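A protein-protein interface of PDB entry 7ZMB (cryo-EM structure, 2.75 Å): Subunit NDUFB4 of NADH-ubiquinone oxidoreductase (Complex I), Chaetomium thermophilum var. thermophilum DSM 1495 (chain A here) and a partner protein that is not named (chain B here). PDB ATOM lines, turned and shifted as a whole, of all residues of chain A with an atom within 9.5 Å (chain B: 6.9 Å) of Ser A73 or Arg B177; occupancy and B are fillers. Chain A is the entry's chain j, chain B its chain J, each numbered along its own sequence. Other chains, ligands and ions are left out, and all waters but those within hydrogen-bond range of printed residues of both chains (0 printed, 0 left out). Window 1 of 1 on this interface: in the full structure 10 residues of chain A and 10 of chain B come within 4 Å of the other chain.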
ATOM      1  N   THR A  57     -20.730  13.410  28.023  1.00  0.00           N
ATOM      2  CA  THR A  57     -21.754  14.178  27.320  1.00  0.00           C
ATOM      3  C   THR A  57     -22.031  15.485  28.037  1.00  0.00           C
ATOM      4  O   THR A  57     -23.181  15.873  28.245  1.00  0.00           O
ATOM      5  CB  THR A  57     -23.051  13.385  27.174  1.00  0.00           C
ATOM      6  OG1 THR A  57     -23.519  12.983  28.468  1.00  0.00           O
ATOM      7  CG2 THR A  57     -22.832  12.153  26.305  1.00  0.00           C
ATOM      8  N   ASP A  58     -20.978  16.197  28.414  1.00  0.00           N
ATOM      9  CA  ASP A  58     -21.099  17.439  29.165  1.00  0.00           C
ATOM     10  C   ASP A  58     -20.725  18.601  28.254  1.00  0.00           C
ATOM     11  O   ASP A  58     -19.633  18.619  27.678  1.00  0.00           O
ATOM     12  CB  ASP A  58     -20.222  17.403  30.413  1.00  0.00           C
ATOM     13  CG  ASP A  58     -20.542  18.509  31.377  1.00  0.00           C
ATOM     14  OD1 ASP A  58     -21.342  19.394  31.025  1.00  0.00           O
ATOM     15  OD2 ASP A  58     -20.020  18.484  32.506  1.00  0.00           O
ATOM     16  N   GLY A  59     -21.634  19.563  28.126  1.00  0.00           N
ATOM     17  CA  GLY A  59     -21.510  20.609  27.143  1.00  0.00           C
ATOM     18  C   GLY A  59     -21.840  20.186  25.732  1.00  0.00           C
ATOM     19  O   GLY A  59     -21.691  20.993  24.810  1.00  0.00           O
ATOM     20  N   LEU A  60     -22.295  18.949  25.533  1.00  0.00           N
ATOM     21  CA  LEU A  60     -22.421  18.411  24.184  1.00  0.00           C
ATOM     22  C   LEU A  60     -23.639  18.974  23.464  1.00  0.00           C
ATOM     23  O   LEU A  60     -23.587  19.218  22.256  1.00  0.00           O
ATOM     24  CB  LEU A  60     -22.479  16.883  24.240  1.00  0.00           C
ATOM     25  CG  LEU A  60     -22.818  16.094  22.975  1.00  0.00           C
ATOM     26  CD1 LEU A  60     -21.954  16.525  21.795  1.00  0.00           C
ATOM     27  CD2 LEU A  60     -22.666  14.615  23.244  1.00  0.00           C
ATOM     28  N   TRP A  61     -24.736  19.196  24.179  1.00  0.00           N
ATOM     29  CA  TRP A  61     -25.978  19.635  23.564  1.00  0.00           C
ATOM     30  C   TRP A  61     -26.468  20.945  24.168  1.00  0.00           C
ATOM     31  O   TRP A  61     -26.168  21.266  25.320  1.00  0.00           O
ATOM     32  CB  TRP A  61     -27.060  18.577  23.711  1.00  0.00           C
ATOM     33  CG  TRP A  61     -26.679  17.268  23.137  1.00  0.00           C
ATOM     34  CD1 TRP A  61     -26.232  17.027  21.877  1.00  0.00           C
ATOM     35  CD2 TRP A  61     -26.705  16.004  23.801  1.00  0.00           C
ATOM     36  NE1 TRP A  61     -25.979  15.693  21.713  1.00  0.00           N
ATOM     37  CE2 TRP A  61     -26.263  15.041  22.881  1.00  0.00           C
ATOM     38  CE3 TRP A  61     -27.067  15.594  25.085  1.00  0.00           C
ATOM     39  CZ2 TRP A  61     -26.173  13.695  23.200  1.00  0.00           C
ATOM     40  CZ3 TRP A  61     -26.975  14.263  25.402  1.00  0.00           C
ATOM     41  CH2 TRP A  61     -26.529  13.325  24.465  1.00  0.00           C
ATOM     42  N   ASP A  62     -27.221  21.699  23.371  1.00  0.00           N
ATOM     43  CA  ASP A  62     -27.865  22.928  23.836  1.00  0.00           C
ATOM     44  C   ASP A  62     -28.975  23.288  22.864  1.00  0.00           C
ATOM     45  O   ASP A  62     -28.713  23.473  21.675  1.00  0.00           O
ATOM     46  CB  ASP A  62     -26.864  24.070  23.947  1.00  0.00           C
ATOM     47  CG  ASP A  62     -27.536  25.403  24.190  1.00  0.00           C
ATOM     48  OD1 ASP A  62     -28.413  25.471  25.078  1.00  0.00           O
ATOM     49  OD2 ASP A  62     -27.191  26.384  23.499  1.00  0.00           O
ATOM     50  N   LEU A  63     -30.204  23.392  23.360  1.00  0.00           N
ATOM     51  CA  LEU A  63     -31.360  23.638  22.511  1.00  0.00           C
ATOM     52  C   LEU A  63     -31.711  25.106  22.368  1.00  0.00           C
ATOM     53  O   LEU A  63     -32.565  25.432  21.540  1.00  0.00           O
ATOM     54  CB  LEU A  63     -32.593  22.912  23.051  1.00  0.00           C
ATOM     55  CG  LEU A  63     -32.518  21.490  23.580  1.00  0.00           C
ATOM     56  CD1 LEU A  63     -33.913  20.999  23.865  1.00  0.00           C
ATOM     57  CD2 LEU A  63     -31.851  20.600  22.572  1.00  0.00           C
ATOM     58  N   ARG A  64     -31.033  25.992  23.104  1.00  0.00           N
ATOM     59  CA  ARG A  64     -31.614  27.256  23.544  1.00  0.00           C
ATOM     60  C   ARG A  64     -32.443  27.957  22.479  1.00  0.00           C
ATOM     61  O   ARG A  64     -33.624  28.248  22.691  1.00  0.00           O
ATOM     62  CB  ARG A  64     -30.519  28.201  24.043  1.00  0.00           C
ATOM     63  CG  ARG A  64     -31.091  29.428  24.740  1.00  0.00           C
ATOM     64  CD  ARG A  64     -31.560  29.078  26.137  1.00  0.00           C
ATOM     65  NE  ARG A  64     -32.513  30.048  26.672  1.00  0.00           N
ATOM     66  CZ  ARG A  64     -33.668  29.721  27.240  1.00  0.00           C
ATOM     67  NH1 ARG A  64     -34.465  30.663  27.702  1.00  0.00           N
ATOM     68  NH2 ARG A  64     -34.014  28.450  27.353  1.00  0.00           N
ATOM     69  N   ALA A  65     -31.836  28.271  21.341  1.00  0.00           N
ATOM     70  CA  ALA A  65     -32.562  28.919  20.261  1.00  0.00           C
ATOM     71  C   ALA A  65     -32.113  28.381  18.915  1.00  0.00           C
ATOM     72  O   ALA A  65     -32.076  29.111  17.921  1.00  0.00           O
ATOM     73  CB  ALA A  65     -32.395  30.436  20.319  1.00  0.00           C
ATOM     74  N   LYS A  66     -31.768  27.100  18.857  1.00  0.00           N
ATOM     75  CA  LYS A  66     -31.274  26.518  17.615  1.00  0.00           C
ATOM     76  C   LYS A  66     -32.420  26.419  16.619  1.00  0.00           C
ATOM     77  O   LYS A  66     -33.390  25.689  16.841  1.00  0.00           O
ATOM     78  CB  LYS A  66     -30.641  25.154  17.874  1.00  0.00           C
ATOM     79  CG  LYS A  66     -29.746  25.112  19.091  1.00  0.00           C
ATOM     80  CD  LYS A  66     -28.445  25.831  18.822  1.00  0.00           C
ATOM     81  CE  LYS A  66     -27.308  25.279  19.650  1.00  0.00           C
ATOM     82  NZ  LYS A  66     -27.178  23.798  19.498  1.00  0.00           N
ATOM     83  N   ARG A  67     -32.310  27.151  15.518  1.00  0.00           N
ATOM     84  CA  ARG A  67     -33.370  27.212  14.523  1.00  0.00           C
ATOM     85  C   ARG A  67     -33.253  26.042  13.551  1.00  0.00           C
ATOM     86  O   ARG A  67     -32.462  25.115  13.739  1.00  0.00           O
ATOM     87  CB  ARG A  67     -33.323  28.535  13.774  1.00  0.00           C
ATOM     88  CG  ARG A  67     -34.020  29.668  14.453  1.00  0.00           C
ATOM     89  CD  ARG A  67     -33.043  30.537  15.181  1.00  0.00           C
ATOM     90  NE  ARG A  67     -32.168  31.256  14.262  1.00  0.00           N
ATOM     91  CZ  ARG A  67     -32.517  32.355  13.603  1.00  0.00           C
ATOM     92  NH1 ARG A  67     -33.740  32.845  13.726  1.00  0.00           N
ATOM     93  NH2 ARG A  67     -31.652  32.949  12.794  1.00  0.00           N
ATOM     94  N   GLY A  69     -31.873  24.311  10.312  1.00  0.00           N
ATOM     95  CA  GLY A  69     -30.579  24.410   9.675  1.00  0.00           C
ATOM     96  C   GLY A  69     -29.399  24.491  10.616  1.00  0.00           C
ATOM     97  O   GLY A  69     -28.268  24.670  10.149  1.00  0.00           O
ATOM     98  N   ASP A  70     -29.619  24.372  11.923  1.00  0.00           N
ATOM     99  CA  ASP A  70     -28.547  24.371  12.904  1.00  0.00           C
ATOM    100  C   ASP A  70     -28.658  23.114  13.758  1.00  0.00           C
ATOM    101  O   ASP A  70     -29.693  22.445  13.782  1.00  0.00           O
ATOM    102  CB  ASP A  70     -28.585  25.628  13.784  1.00  0.00           C
ATOM    103  CG  ASP A  70     -27.303  25.830  14.575  1.00  0.00           C
ATOM    104  OD1 ASP A  70     -26.619  24.832  14.885  1.00  0.00           O
ATOM    105  OD2 ASP A  70     -26.975  26.994  14.887  1.00  0.00           O
ATOM    106  N   LEU A  71     -27.578  22.801  14.462  1.00  0.00           N
ATOM    107  CA  LEU A  71     -27.469  21.547  15.189  1.00  0.00           C
ATOM    108  C   LEU A  71     -27.668  21.748  16.687  1.00  0.00           C
ATOM    109  O   LEU A  71     -27.273  22.766  17.259  1.00  0.00           O
ATOM    110  CB  LEU A  71     -26.111  20.895  14.934  1.00  0.00           C
ATOM    111  CG  LEU A  71     -25.661  20.858  13.472  1.00  0.00           C
ATOM    112  CD1 LEU A  71     -24.342  20.118  13.340  1.00  0.00           C
ATOM    113  CD2 LEU A  71     -26.726  20.224  12.592  1.00  0.00           C
ATOM    114  N   ILE A  72     -28.294  20.752  17.314  1.00  0.00           N
ATOM    115  CA  ILE A  72     -28.374  20.708  18.770  1.00  0.00           C
ATOM    116  C   ILE A  72     -26.982  20.622  19.383  1.00  0.00           C
ATOM    117  O   ILE A  72     -26.702  21.244  20.415  1.00  0.00           O
ATOM    118  CB  ILE A  72     -29.250  19.523  19.216  1.00  0.00           C
ATOM    119  CG1 ILE A  72     -30.686  19.689  18.728  1.00  0.00           C
ATOM    120  CG2 ILE A  72     -29.176  19.345  20.711  1.00  0.00           C
ATOM    121  CD1 ILE A  72     -31.631  18.657  19.277  1.00  0.00           C
ATOM    122  N   SER A  73     -26.096  19.840  18.773  1.00  0.00           N
ATOM    123  CA  SER A  73     -24.789  19.597  19.361  1.00  0.00           C
ATOM    124  C   SER A  73     -23.936  20.856  19.336  1.00  0.00           C
ATOM    125  O   SER A  73     -24.097  21.729  18.482  1.00  0.00           O
ATOM    126  CB  SER A  73     -24.068  18.473  18.626  1.00  0.00           C
ATOM    127  OG  SER A  73     -22.700  18.443  18.984  1.00  0.00           O
ATOM    128  N   GLU A  74     -23.023  20.947  20.301  1.00  0.00           N
ATOM    129  CA  GLU A  74     -22.073  22.046  20.371  1.00  0.00           C
ATOM    130  C   GLU A  74     -20.625  21.585  20.406  1.00  0.00           C
ATOM    131  O   GLU A  74     -19.722  22.432  20.386  1.00  0.00           O
ATOM    132  CB  GLU A  74     -22.353  22.924  21.598  1.00  0.00           C
ATOM    133  CG  GLU A  74     -23.566  23.826  21.461  1.00  0.00           C
ATOM    134  CD  GLU A  74     -23.704  24.788  22.624  1.00  0.00           C
ATOM    135  OE1 GLU A  74     -22.969  24.631  23.621  1.00  0.00           O
ATOM    136  OE2 GLU A  74     -24.538  25.714  22.536  1.00  0.00           O
ATOM    137  N   ARG A  75     -20.371  20.284  20.459  1.00  0.00           N
ATOM    138  CA  ARG A  75     -19.010  19.780  20.549  1.00  0.00           C
ATOM    139  C   ARG A  75     -18.857  18.492  19.746  1.00  0.00           C
ATOM    140  O   ARG A  75     -19.815  17.740  19.577  1.00  0.00           O
ATOM    141  CB  ARG A  75     -18.628  19.552  22.015  1.00  0.00           C
ATOM    142  CG  ARG A  75     -17.245  18.966  22.224  1.00  0.00           C
ATOM    143  CD  ARG A  75     -16.874  18.936  23.698  1.00  0.00           C
ATOM    144  NE  ARG A  75     -18.007  18.589  24.553  1.00  0.00           N
ATOM    145  CZ  ARG A  75     -18.511  17.364  24.671  1.00  0.00           C
ATOM    146  NH1 ARG A  75     -19.540  17.146  25.478  1.00  0.00           N
ATOM    147  NH2 ARG A  75     -17.989  16.356  23.986  1.00  0.00           N
ATOM    148  OXT ARG A  75     -17.781  18.176  19.240  1.00  0.00           O
ATOM    149  N   GLU B 164     -14.679  25.937  27.408  1.00  0.00           N
ATOM    150  CA  GLU B 164     -15.499  26.938  26.753  1.00  0.00           C
ATOM    151  C   GLU B 164     -16.859  26.311  26.501  1.00  0.00           C
ATOM    152  O   GLU B 164     -16.947  25.130  26.162  1.00  0.00           O
ATOM    153  CB  GLU B 164     -14.837  27.407  25.456  1.00  0.00           C
ATOM    154  CG  GLU B 164     -15.354  28.708  24.901  1.00  0.00           C
ATOM    155  CD  GLU B 164     -14.795  28.995  23.521  1.00  0.00           C
ATOM    156  OE1 GLU B 164     -15.277  29.934  22.857  1.00  0.00           O
ATOM    157  OE2 GLU B 164     -13.866  28.276  23.098  1.00  0.00           O
ATOM    158  N   LYS B 169     -19.508  31.264  27.284  1.00  0.00           N
ATOM    159  CA  LYS B 169     -19.645  31.594  25.871  1.00  0.00           C
ATOM    160  C   LYS B 169     -19.021  32.963  25.670  1.00  0.00           C
ATOM    161  O   LYS B 169     -19.704  33.989  25.780  1.00  0.00           O
ATOM    162  CB  LYS B 169     -21.112  31.576  25.441  1.00  0.00           C
ATOM    163  CG  LYS B 169     -21.781  30.238  25.696  1.00  0.00           C
ATOM    164  CD  LYS B 169     -22.666  29.811  24.536  1.00  0.00           C
ATOM    165  CE  LYS B 169     -23.807  30.787  24.298  1.00  0.00           C
ATOM    166  NZ  LYS B 169     -24.782  30.784  25.423  1.00  0.00           N
ATOM    167  N   GLY B 172     -16.880  35.800  20.512  1.00  0.00           N
ATOM    168  CA  GLY B 172     -16.254  34.923  19.551  1.00  0.00           C
ATOM    169  C   GLY B 172     -16.615  33.462  19.688  1.00  0.00           C
ATOM    170  O   GLY B 172     -16.045  32.635  18.967  1.00  0.00           O
ATOM    171  N   TYR B 173     -17.533  33.114  20.595  1.00  0.00           N
ATOM    172  CA  TYR B 173     -17.996  31.733  20.685  1.00  0.00           C
ATOM    173  C   TYR B 173     -18.667  31.290  19.395  1.00  0.00           C
ATOM    174  O   TYR B 173     -18.430  30.179  18.914  1.00  0.00           O
ATOM    175  CB  TYR B 173     -18.963  31.567  21.855  1.00  0.00           C
ATOM    176  CG  TYR B 173     -19.187  30.125  22.261  1.00  0.00           C
ATOM    177  CD1 TYR B 173     -18.198  29.402  22.899  1.00  0.00           C
ATOM    178  CD2 TYR B 173     -20.380  29.486  21.979  1.00  0.00           C
ATOM    179  CE1 TYR B 173     -18.394  28.094  23.261  1.00  0.00           C
ATOM    180  CE2 TYR B 173     -20.585  28.178  22.332  1.00  0.00           C
ATOM    181  CZ  TYR B 173     -19.588  27.484  22.978  1.00  0.00           C
ATOM    182  OH  TYR B 173     -19.783  26.171  23.339  1.00  0.00           O
ATOM    183  N   TYR B 174     -19.507  32.148  18.817  1.00  0.00           N
ATOM    184  CA  TYR B 174     -20.300  31.738  17.665  1.00  0.00           C
ATOM    185  C   TYR B 174     -19.471  31.687  16.389  1.00  0.00           C
ATOM    186  O   TYR B 174     -19.676  30.803  15.550  1.00  0.00           O
ATOM    187  CB  TYR B 174     -21.498  32.669  17.501  1.00  0.00           C
ATOM    188  CG  TYR B 174     -22.617  32.359  18.470  1.00  0.00           C
ATOM    189  CD1 TYR B 174     -22.512  31.294  19.355  1.00  0.00           C
ATOM    190  CD2 TYR B 174     -23.774  33.120  18.494  1.00  0.00           C
ATOM    191  CE1 TYR B 174     -23.527  31.001  20.239  1.00  0.00           C
ATOM    192  CE2 TYR B 174     -24.796  32.833  19.377  1.00  0.00           C
ATOM    193  CZ  TYR B 174     -24.668  31.773  20.247  1.00  0.00           C
ATOM    194  OH  TYR B 174     -25.681  31.480  21.129  1.00  0.00           O
ATOM    195  N   GLU B 175     -18.535  32.623  16.219  1.00  0.00           N
ATOM    196  CA  GLU B 175     -17.695  32.606  15.026  1.00  0.00           C
ATOM    197  C   GLU B 175     -16.841  31.347  14.972  1.00  0.00           C
ATOM    198  O   GLU B 175     -16.709  30.719  13.915  1.00  0.00           O
ATOM    199  CB  GLU B 175     -16.816  33.856  14.984  1.00  0.00           C
ATOM    200  N   ARG B 176     -16.256  30.957  16.106  1.00  0.00           N
ATOM    201  CA  ARG B 176     -15.432  29.755  16.146  1.00  0.00           C
ATOM    202  C   ARG B 176     -16.269  28.482  16.168  1.00  0.00           C
ATOM    203  O   ARG B 176     -15.827  27.450  15.650  1.00  0.00           O
ATOM    204  CB  ARG B 176     -14.502  29.795  17.357  1.00  0.00           C
ATOM    205  CG  ARG B 176     -13.227  30.585  17.121  1.00  0.00           C
ATOM    206  CD  ARG B 176     -12.207  30.339  18.228  1.00  0.00           C
ATOM    207  NE  ARG B 176     -12.747  30.564  19.569  1.00  0.00           N
ATOM    208  CZ  ARG B 176     -13.229  31.722  20.016  1.00  0.00           C
ATOM    209  NH1 ARG B 176     -13.697  31.805  21.253  1.00  0.00           N
ATOM    210  NH2 ARG B 176     -13.224  32.804  19.248  1.00  0.00           N
ATOM    211  N   ARG B 177     -17.463  28.530  16.762  1.00  0.00           N
ATOM    212  CA  ARG B 177     -18.310  27.343  16.816  1.00  0.00           C
ATOM    213  C   ARG B 177     -18.710  26.892  15.419  1.00  0.00           C
ATOM    214  O   ARG B 177     -18.753  25.690  15.136  1.00  0.00           O
ATOM    215  CB  ARG B 177     -19.549  27.617  17.665  1.00  0.00           C
ATOM    216  CG  ARG B 177     -20.458  26.422  17.859  1.00  0.00           C
ATOM    217  CD  ARG B 177     -21.658  26.789  18.709  1.00  0.00           C
ATOM    218  NE  ARG B 177     -22.803  25.926  18.434  1.00  0.00           N
ATOM    219  CZ  ARG B 177     -23.639  26.099  17.415  1.00  0.00           C
ATOM    220  NH1 ARG B 177     -24.654  25.265  17.240  1.00  0.00           N
ATOM    221  NH2 ARG B 177     -23.462  27.108  16.574  1.00  0.00           N
ATOM    222  N   ALA B 178     -19.013  27.844  14.535  1.00  0.00           N
ATOM    223  CA  ALA B 178     -19.363  27.492  13.165  1.00  0.00           C
ATOM    224  C   ALA B 178     -18.208  26.785  12.470  1.00  0.00           C
ATOM    225  O   ALA B 178     -18.413  25.790  11.765  1.00  0.00           O
ATOM    226  CB  ALA B 178     -19.772  28.743  12.390  1.00  0.00           C
ATOM    227  N   GLN B 179     -16.986  27.280  12.658  1.00  0.00           N
ATOM    228  CA  GLN B 179     -15.828  26.627  12.059  1.00  0.00           C
ATOM    229  C   GLN B 179     -15.597  25.247  12.659  1.00  0.00           C
ATOM    230  O   GLN B 179     -15.309  24.290  11.933  1.00  0.00           O
ATOM    231  CB  GLN B 179     -14.585  27.500  12.228  1.00  0.00           C
ATOM    232  CG  GLN B 179     -14.633  28.804  11.452  1.00  0.00           C
ATOM    233  CD  GLN B 179     -13.392  29.649  11.660  1.00  0.00           C
ATOM    234  OE1 GLN B 179     -12.510  29.296  12.442  1.00  0.00           O
ATOM    235  NE2 GLN B 179     -13.320  30.775  10.961  1.00  0.00           N
ATOM    236  N   ARG B 180     -15.725  25.123  13.982  1.00  0.00           N
ATOM    237  CA  ARG B 180     -15.464  23.843  14.633  1.00  0.00           C
ATOM    238  C   ARG B 180     -16.442  22.774  14.169  1.00  0.00           C
ATOM    239  O   ARG B 180     -16.052  21.626  13.929  1.00  0.00           O
ATOM    240  CB  ARG B 180     -15.524  24.005  16.151  1.00  0.00           C
ATOM    241  CG  ARG B 180     -15.122  22.757  16.918  1.00  0.00           C
ATOM    242  CD  ARG B 180     -14.719  23.089  18.345  1.00  0.00           C
ATOM    243  NE  ARG B 180     -15.561  24.130  18.923  1.00  0.00           N
ATOM    244  CZ  ARG B 180     -16.676  23.892  19.606  1.00  0.00           C
ATOM    245  NH1 ARG B 180     -17.381  24.899  20.098  1.00  0.00           N
ATOM    246  NH2 ARG B 180     -17.084  22.646  19.797  1.00  0.00           N
ATOM    247  N   LEU B 181     -17.722  23.131  14.040  1.00  0.00           N
ATOM    248  CA  LEU B 181     -18.712  22.170  13.562  1.00  0.00           C
ATOM    249  C   LEU B 181     -18.429  21.757  12.123  1.00  0.00           C
ATOM    250  O   LEU B 181     -18.601  20.589  11.760  1.00  0.00           O
ATOM    251  CB  LEU B 181     -20.118  22.757  13.685  1.00  0.00           C
ATOM    252  CG  LEU B 181     -20.888  22.510  14.986  1.00  0.00           C
ATOM    253  CD1 LEU B 181     -21.183  21.032  15.145  1.00  0.00           C
ATOM    254  CD2 LEU B 181     -20.137  23.034  16.198  1.00  0.00           C
ATOM    255  N   LYS B 182     -18.002  22.707  11.288  1.00  0.00           N
ATOM    256  CA  LYS B 182     -17.728  22.399   9.889  1.00  0.00           C
ATOM    257  C   LYS B 182     -16.592  21.394   9.753  1.00  0.00           C
ATOM    258  O   LYS B 182     -16.670  20.463   8.944  1.00  0.00           O
ATOM    259  CB  LYS B 182     -17.405  23.683   9.127  1.00  0.00           C
ATOM    260  CG  LYS B 182     -17.158  23.485   7.642  1.00  0.00           C
ATOM    261  CD  LYS B 182     -18.432  23.091   6.919  1.00  0.00           C
ATOM    262  CE  LYS B 182     -18.189  22.925   5.428  1.00  0.00           C
ATOM    263  NZ  LYS B 182     -17.834  24.217   4.778  1.00  0.00           N
ATOM    264  N   LYS B 184     -15.759  19.067  11.651  1.00  0.00           N
ATOM    265  CA  LYS B 184     -16.102  17.757  12.190  1.00  0.00           C
ATOM    266  C   LYS B 184     -17.258  17.086  11.471  1.00  0.00           C
ATOM    267  O   LYS B 184     -17.171  15.898  11.154  1.00  0.00           O
ATOM    268  CB  LYS B 184     -16.443  17.868  13.681  1.00  0.00           C
ATOM    269  CG  LYS B 184     -16.520  16.529  14.390  1.00  0.00           C
ATOM    270  CD  LYS B 184     -16.862  16.694  15.860  1.00  0.00           C
ATOM    271  CE  LYS B 184     -16.628  15.402  16.623  1.00  0.00           C
ATOM    272  NZ  LYS B 184     -17.491  14.299  16.121  1.00  0.00           N
ATOM    273  N   TYR B 185     -18.343  17.812  11.203  1.00  0.00           N
ATOM    274  CA  TYR B 185     -19.515  17.234  10.564  1.00  0.00           C
ATOM    275  C   TYR B 185     -19.667  17.632   9.104  1.00  0.00           C
ATOM    276  O   TYR B 185     -20.512  17.057   8.410  1.00  0.00           O
ATOM    277  CB  TYR B 185     -20.788  17.631  11.328  1.00  0.00           C
ATOM    278  CG  TYR B 185     -20.800  17.196  12.777  1.00  0.00           C
ATOM    279  CD1 TYR B 185     -20.022  16.132  13.214  1.00  0.00           C
ATOM    280  CD2 TYR B 185     -21.587  17.855  13.710  1.00  0.00           C
ATOM    281  CE1 TYR B 185     -20.032  15.736  14.537  1.00  0.00           C
ATOM    282  CE2 TYR B 185     -21.603  17.468  15.033  1.00  0.00           C
ATOM    283  CZ  TYR B 185     -20.824  16.409  15.443  1.00  0.00           C
ATOM    284  OH  TYR B 185     -20.840  16.021  16.762  1.00  0.00           O
ATOM    285  N   ILE B 189     -23.119  26.139   8.668  1.00  0.00           N
ATOM    286  CA  ILE B 189     -24.143  26.677   9.557  1.00  0.00           C
ATOM    287  C   ILE B 189     -24.738  27.927   8.926  1.00  0.00           C
ATOM    288  O   ILE B 189     -24.016  28.874   8.597  1.00  0.00           O
ATOM    289  CB  ILE B 189     -23.568  26.978  10.946  1.00  0.00           C
ATOM    290  CG1 ILE B 189     -23.131  25.684  11.631  1.00  0.00           C
ATOM    291  CG2 ILE B 189     -24.588  27.717  11.794  1.00  0.00           C
ATOM    292  CD1 ILE B 189     -24.265  24.709  11.864  1.00  0.00           C
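CE of Lys A66 touches NH1 of Arg B177 (3.6 Å).
CD1 of Ile B189 touches OD1 of Asp A70, at 3.8 Å.
Leu A71 touches Arg B177.
Leu A71 touches Leu B181 (CD1 to CD1, 3.8 Å).
NH1 of Arg B177 touches O of Ser A73, at 3.8 Å.
OH of Tyr B185 touches OG of Ser A73, 3.8 Å away.
Tyr B173 touches Glu A74 (OH to OE1, 3.5 Å).
Glu A74 touches Arg B177 (CG to NE, 3.8 Å).
CA of Arg A75 touches NH2 of Arg B180 (3.5 Å).
Arg A75 touches Lys B184.
The side-chain carboxylate of Asp A70 lies within salt-bridge range of the guanidinium group of Arg B177 (3.1 Å).
NH2 of Arg B180 sits at hydrogen-bond distance from O of Glu A74.
The side-chain hydroxyl (OH) of Tyr B185 lies within hydrogen-bond range of the chain-end carboxylate (O) of Arg A75 (3.5 Å).
Printed residues of chain B within 4 Å of Leu A71: Arg B177 (3.6 Å), Leu B181 (3.8 Å) and Tyr B185 (3.6 Å).
Arg B176 touches none of the printed residues of chain A.
Arg B177 touches five residues of chain A.
Printed residues of chain A within 4 Å of Lys B184: Arg A75 (3.8 Å).
Of the printed residues of chain A, Tyr B185 touches Leu A71 (3.6 Å), Ser A73 (3.8 Å) and Arg A75 (3.5 Å).
The nearest residue of chain B that does not touch Ser A73 is Leu B181 (4.5 Å).
The nearest printed residue of chain A that does not touch Lys B184 is Ser A73 (6.8 Å).
The backbone carbonyl oxygen (O) of Asp A58 lies within hydrogen-bond range of the guanidinium group (NH1) of Arg A75 (2.6 Å).
O of Leu A60 sits close to OG of Ser A73 (3.5 Å).
The backbone carbonyl oxygen of Leu A60 sits at hydrogen-bond distance from the backbone NH of Glu A74 (2.7 Å).
The backbone carbonyl oxygen (O) of Asp A62 lies within hydrogen-bond range of the side-chain amino group (NZ) of Lys A66, 2.7 Å away.
The backbone carbonyl oxygen of Ile A72 is in hydrogen-bond range of the side-chain amino group of Lys A66 (2.8 Å).
The side-chain hydroxyl (OG) of Ser A73 is in hydrogen-bond range of the chain-end carboxylate (O) of Arg A75, 3.0 Å away.
Of the 18 printed residues of chain A, 6 touch a printed residue of chain B.
Along chain A the printed residues that touch a printed residue of chain B span positions 66 to 75.
Of the 16 printed residues of chain B, 7 touch a printed residue of chain A.
Hydrophobic or aromatic side chains of chain B that line the printed part of chain A: Tyr B173, Leu B181, Tyr B185 and Ile B189.
Among the printed residues, Asp or Glu carboxylates within 4 Å of a Lys or Arg side-chain nitrogen of the other chain: Asp A70 with Arg B177 (3.1 Å).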
